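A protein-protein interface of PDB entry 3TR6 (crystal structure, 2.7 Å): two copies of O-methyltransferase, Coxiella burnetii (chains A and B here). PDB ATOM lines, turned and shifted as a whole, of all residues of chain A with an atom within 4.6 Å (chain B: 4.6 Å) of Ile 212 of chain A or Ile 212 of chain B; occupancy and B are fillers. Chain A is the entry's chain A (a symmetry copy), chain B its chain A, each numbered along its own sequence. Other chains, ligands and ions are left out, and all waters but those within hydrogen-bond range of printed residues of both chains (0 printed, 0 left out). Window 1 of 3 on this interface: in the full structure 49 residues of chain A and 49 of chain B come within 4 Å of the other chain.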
ATOM      1  N   LEU A  55      12.279 -27.192 -15.166  1.00  0.00           N
ATOM      2  CA  LEU A  55      13.520 -27.717 -14.616  1.00  0.00           C
ATOM      3  C   LEU A  55      13.289 -29.092 -14.002  1.00  0.00           C
ATOM      4  O   LEU A  55      14.126 -29.983 -14.129  1.00  0.00           O
ATOM      5  CB  LEU A  55      14.081 -26.759 -13.561  1.00  0.00           C
ATOM      6  CG  LEU A  55      15.152 -27.297 -12.603  1.00  0.00           C
ATOM      7  CD1 LEU A  55      16.401 -27.749 -13.358  1.00  0.00           C
ATOM      8  CD2 LEU A  55      15.506 -26.248 -11.558  1.00  0.00           C
ATOM      9  N   ILE A 210      22.126 -28.094  -3.559  1.00  0.00           N
ATOM     10  CA  ILE A 210      22.296 -26.850  -4.283  1.00  0.00           C
ATOM     11  C   ILE A 210      20.980 -26.095  -4.156  1.00  0.00           C
ATOM     12  O   ILE A 210      19.918 -26.712  -4.057  1.00  0.00           O
ATOM     13  CB  ILE A 210      22.621 -27.108  -5.764  1.00  0.00           C
ATOM     14  CG1 ILE A 210      23.170 -25.847  -6.436  1.00  0.00           C
ATOM     15  CG2 ILE A 210      21.394 -27.613  -6.500  1.00  0.00           C
ATOM     16  CD1 ILE A 210      24.570 -25.486  -6.007  1.00  0.00           C
ATOM     17  N   LEU A 211      21.044 -24.768  -4.133  1.00  0.00           N
ATOM     18  CA  LEU A 211      19.831 -23.961  -4.087  1.00  0.00           C
ATOM     19  C   LEU A 211      19.705 -23.120  -5.355  1.00  0.00           C
ATOM     20  O   LEU A 211      20.450 -22.156  -5.554  1.00  0.00           O
ATOM     21  CB  LEU A 211      19.821 -23.071  -2.844  1.00  0.00           C
ATOM     22  CG  LEU A 211      18.469 -22.515  -2.389  1.00  0.00           C
ATOM     23  CD1 LEU A 211      18.584 -21.936  -0.987  1.00  0.00           C
ATOM     24  CD2 LEU A 211      17.928 -21.473  -3.362  1.00  0.00           C
ATOM     25  N   ILE A 212      18.762 -23.496  -6.211  1.00  0.00           N
ATOM     26  CA  ILE A 212      18.571 -22.827  -7.489  1.00  0.00           C
ATOM     27  C   ILE A 212      17.603 -21.659  -7.350  1.00  0.00           C
ATOM     28  O   ILE A 212      16.483 -21.831  -6.869  1.00  0.00           O
ATOM     29  CB  ILE A 212      18.011 -23.792  -8.561  1.00  0.00           C
ATOM     30  CG1 ILE A 212      18.745 -25.136  -8.533  1.00  0.00           C
ATOM     31  CG2 ILE A 212      18.096 -23.164  -9.941  1.00  0.00           C
ATOM     32  CD1 ILE A 212      20.134 -25.085  -9.113  1.00  0.00           C
ATOM     33  N   PRO A 213      18.034 -20.463  -7.775  1.00  0.00           N
ATOM     34  CA  PRO A 213      17.175 -19.276  -7.748  1.00  0.00           C
ATOM     35  C   PRO A 213      16.194 -19.260  -8.925  1.00  0.00           C
ATOM     36  O   PRO A 213      16.158 -18.306  -9.697  1.00  0.00           O
ATOM     37  CB  PRO A 213      18.177 -18.126  -7.872  1.00  0.00           C
ATOM     38  CG  PRO A 213      19.285 -18.705  -8.677  1.00  0.00           C
ATOM     39  CD  PRO A 213      19.390 -20.149  -8.257  1.00  0.00           C
ATOM     40  N   ILE A 214      15.415 -20.325  -9.060  1.00  0.00           N
ATOM     41  CA  ILE A 214      14.344 -20.365 -10.039  1.00  0.00           C
ATOM     42  C   ILE A 214      13.036 -20.629  -9.296  1.00  0.00           C
ATOM     43  O   ILE A 214      13.031 -21.327  -8.279  1.00  0.00           O
ATOM     44  CB  ILE A 214      14.600 -21.436 -11.122  1.00  0.00           C
ATOM     45  CG1 ILE A 214      13.870 -21.071 -12.415  1.00  0.00           C
ATOM     46  CG2 ILE A 214      14.199 -22.818 -10.627  1.00  0.00           C
ATOM     47  CD1 ILE A 214      14.243 -21.945 -13.582  1.00  0.00           C
ATOM     48  N   GLY A 217      12.732 -20.338  -5.424  1.00  0.00           N
ATOM     49  CA  GLY A 217      13.889 -21.026  -4.891  1.00  0.00           C
ATOM     50  C   GLY A 217      13.639 -22.518  -4.870  1.00  0.00           C
ATOM     51  O   GLY A 217      12.616 -22.985  -4.363  1.00  0.00           O
ATOM     52  N   LEU A 218      14.572 -23.270  -5.437  1.00  0.00           N
ATOM     53  CA  LEU A 218      14.440 -24.713  -5.495  1.00  0.00           C
ATOM     54  C   LEU A 218      15.693 -25.393  -4.955  1.00  0.00           C
ATOM     55  O   LEU A 218      16.745 -25.379  -5.596  1.00  0.00           O
ATOM     56  CB  LEU A 218      14.160 -25.163  -6.930  1.00  0.00           C
ATOM     57  CG  LEU A 218      13.874 -26.660  -7.069  1.00  0.00           C
ATOM     58  CD1 LEU A 218      12.541 -27.027  -6.419  1.00  0.00           C
ATOM     59  CD2 LEU A 218      13.897 -27.061  -8.529  1.00  0.00           C
ATOM     60  N   LEU A 220      17.832 -28.609  -4.207  1.00  0.00           N
ATOM     61  CA  LEU A 220      17.979 -29.989  -4.642  1.00  0.00           C
ATOM     62  C   LEU A 220      18.926 -30.710  -3.694  1.00  0.00           C
ATOM     63  O   LEU A 220      20.014 -30.222  -3.409  1.00  0.00           O
ATOM     64  CB  LEU A 220      18.513 -30.056  -6.068  1.00  0.00           C
ATOM     65  CG  LEU A 220      17.735 -29.237  -7.092  1.00  0.00           C
ATOM     66  CD1 LEU A 220      18.391 -29.319  -8.464  1.00  0.00           C
ATOM     67  CD2 LEU A 220      16.283 -29.688  -7.157  1.00  0.00           C
ATOM     68  N   LEU B  55      26.866 -26.726  -8.893  1.00  0.00           N
ATOM     69  CA  LEU B  55      25.738 -27.283  -9.625  1.00  0.00           C
ATOM     70  C   LEU B  55      26.220 -28.307 -10.643  1.00  0.00           C
ATOM     71  O   LEU B  55      25.584 -29.340 -10.840  1.00  0.00           O
ATOM     72  CB  LEU B  55      24.961 -26.167 -10.330  1.00  0.00           C
ATOM     73  CG  LEU B  55      23.988 -26.569 -11.446  1.00  0.00           C
ATOM     74  CD1 LEU B  55      22.882 -27.483 -10.922  1.00  0.00           C
ATOM     75  CD2 LEU B  55      23.396 -25.332 -12.106  1.00  0.00           C
ATOM     76  N   ILE B 210      17.014 -25.774 -20.491  1.00  0.00           N
ATOM     77  CA  ILE B 210      16.622 -24.892 -19.408  1.00  0.00           C
ATOM     78  C   ILE B 210      17.754 -23.889 -19.239  1.00  0.00           C
ATOM     79  O   ILE B 210      18.915 -24.213 -19.496  1.00  0.00           O
ATOM     80  CB  ILE B 210      16.406 -25.677 -18.103  1.00  0.00           C
ATOM     81  CG1 ILE B 210      15.637 -24.840 -17.077  1.00  0.00           C
ATOM     82  CG2 ILE B 210      17.733 -26.136 -17.530  1.00  0.00           C
ATOM     83  CD1 ILE B 210      14.179 -24.648 -17.413  1.00  0.00           C
ATOM     84  N   LEU B 211      17.424 -22.668 -18.832  1.00  0.00           N
ATOM     85  CA  LEU B 211      18.447 -21.662 -18.573  1.00  0.00           C
ATOM     86  C   LEU B 211      18.444 -21.272 -17.097  1.00  0.00           C
ATOM     87  O   LEU B 211      17.529 -20.596 -16.621  1.00  0.00           O
ATOM     88  CB  LEU B 211      18.236 -20.435 -19.459  1.00  0.00           C
ATOM     89  CG  LEU B 211      19.433 -19.502 -19.662  1.00  0.00           C
ATOM     90  CD1 LEU B 211      19.156 -18.535 -20.804  1.00  0.00           C
ATOM     91  CD2 LEU B 211      19.786 -18.746 -18.386  1.00  0.00           C
ATOM     92  N   ILE B 212      19.473 -21.707 -16.378  1.00  0.00           N
ATOM     93  CA  ILE B 212      19.569 -21.465 -14.945  1.00  0.00           C
ATOM     94  C   ILE B 212      20.276 -20.147 -14.666  1.00  0.00           C
ATOM     95  O   ILE B 212      21.392 -19.924 -15.138  1.00  0.00           O
ATOM     96  CB  ILE B 212      20.347 -22.593 -14.227  1.00  0.00           C
ATOM     97  CG1 ILE B 212      19.897 -23.973 -14.714  1.00  0.00           C
ATOM     98  CG2 ILE B 212      20.184 -22.477 -12.721  1.00  0.00           C
ATOM     99  CD1 ILE B 212      18.548 -24.394 -14.197  1.00  0.00           C
ATOM    100  N   PRO B 213      19.629 -19.265 -13.890  1.00  0.00           N
ATOM    101  CA  PRO B 213      20.230 -17.986 -13.501  1.00  0.00           C
ATOM    102  C   PRO B 213      21.226 -18.156 -12.351  1.00  0.00           C
ATOM    103  O   PRO B 213      21.097 -17.519 -11.309  1.00  0.00           O
ATOM    104  CB  PRO B 213      19.022 -17.166 -13.046  1.00  0.00           C
ATOM    105  CG  PRO B 213      18.081 -18.185 -12.510  1.00  0.00           C
ATOM    106  CD  PRO B 213      18.254 -19.404 -13.379  1.00  0.00           C
ATOM    107  N   ILE B 214      22.209 -19.027 -12.543  1.00  0.00           N
ATOM    108  CA  ILE B 214      23.299 -19.168 -11.594  1.00  0.00           C
ATOM    109  C   ILE B 214      24.606 -18.907 -12.337  1.00  0.00           C
ATOM    110  O   ILE B 214      24.718 -19.222 -13.524  1.00  0.00           O
ATOM    111  CB  ILE B 214      23.300 -20.560 -10.926  1.00  0.00           C
ATOM    112  CG1 ILE B 214      23.985 -20.496  -9.560  1.00  0.00           C
ATOM    113  CG2 ILE B 214      23.953 -21.596 -11.828  1.00  0.00           C
ATOM    114  CD1 ILE B 214      23.834 -21.757  -8.753  1.00  0.00           C
ATOM    115  N   GLY B 217      24.714 -17.320 -15.893  1.00  0.00           N
ATOM    116  CA  GLY B 217      23.702 -18.016 -16.658  1.00  0.00           C
ATOM    117  C   GLY B 217      24.246 -19.339 -17.155  1.00  0.00           C
ATOM    118  O   GLY B 217      25.324 -19.400 -17.750  1.00  0.00           O
ATOM    119  N   LEU B 218      23.503 -20.405 -16.895  1.00  0.00           N
ATOM    120  CA  LEU B 218      23.924 -21.730 -17.302  1.00  0.00           C
ATOM    121  C   LEU B 218      22.815 -22.436 -18.077  1.00  0.00           C
ATOM    122  O   LEU B 218      21.805 -22.842 -17.502  1.00  0.00           O
ATOM    123  CB  LEU B 218      24.337 -22.555 -16.083  1.00  0.00           C
ATOM    124  CG  LEU B 218      24.923 -23.928 -16.427  1.00  0.00           C
ATOM    125  CD1 LEU B 218      26.280 -23.787 -17.116  1.00  0.00           C
ATOM    126  CD2 LEU B 218      25.031 -24.777 -15.178  1.00  0.00           C
ATOM    127  N   LEU B 220      21.344 -25.596 -19.899  1.00  0.00           N
ATOM    128  CA  LEU B 220      21.492 -27.043 -19.941  1.00  0.00           C
ATOM    129  C   LEU B 220      20.677 -27.592 -21.103  1.00  0.00           C
ATOM    130  O   LEU B 220      19.504 -27.266 -21.251  1.00  0.00           O
ATOM    131  CB  LEU B 220      21.031 -27.674 -18.633  1.00  0.00           C
ATOM    132  CG  LEU B 220      21.663 -27.093 -17.372  1.00  0.00           C
ATOM    133  CD1 LEU B 220      21.083 -27.746 -16.125  1.00  0.00           C
ATOM    134  CD2 LEU B 220      23.176 -27.239 -17.408  1.00  0.00           C
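N of Leu 218 of chain B is in hydrogen-bond range of O of Ile 212 of chain B (2.8 Å). The backbone carbonyl oxygen (O) of Ile 210 of chain B is in hydrogen-bond range of the backbone NH (N) of Leu 220 of chain B (2.8 Å). N of Leu 218 of chain A sits at hydrogen-bond distance from O of Ile 212 of chain A (2.8 Å). N of Leu 220 of chain A lies within hydrogen-bond range of O of Ile 210 of chain A (2.8 Å).
Leu 55 of chain A touches Ile 210 of chain B. Leu 55 of chain B touches Ile 210 of chain A (N to CD1, 3.9 Å). Ile 212 of chain B touches Ile 212 of chain A. Pro 213 of chain A touches Pro 213 of chain B (CG to O, 3.4 Å).
Of the printed residues of chain B, Ile 210 of chain A touches Leu 55 (3.9 Å). Ile 212 of chain A touches one residue of chain B. Printed residues of chain B within 4 Å of Pro 213 of chain A: Pro 213 (3.4 Å). Of the printed residues of chain A, Leu 55 of chain B touches Ile 210 (3.9 Å). Of the printed residues of chain A, Ile 210 of chain B touches Leu 55. The nearest residue of chain B that does not touch Ile 212 of chain A is Leu 55 of chain B (4.1 Å).
Hydrophobic or aromatic side chains of chain A that line the printed part of chain B: Ile 210, Ile 212 and Pro 213. Of the 9 printed residues of chain B, 4 touch a printed residue of chain A.
Leu 55 of chain A touches Ile 210 of chain B, and with the chains exchanged Ile 210 of chain A touches Leu 55 of chain B. Ile 212 of chain A touches its own counterpart, Ile 212 of chain B. Pro 213 of chain B touches its own counterpart, Pro 213 of chain A. Positions printed for both chains: 55, 210, 211, 212, 213, 214, 217, 218 and 220. Of the 4 pairs that touch across the chains among the printed residues, 4 have their exchanged pair printed and touching as well.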
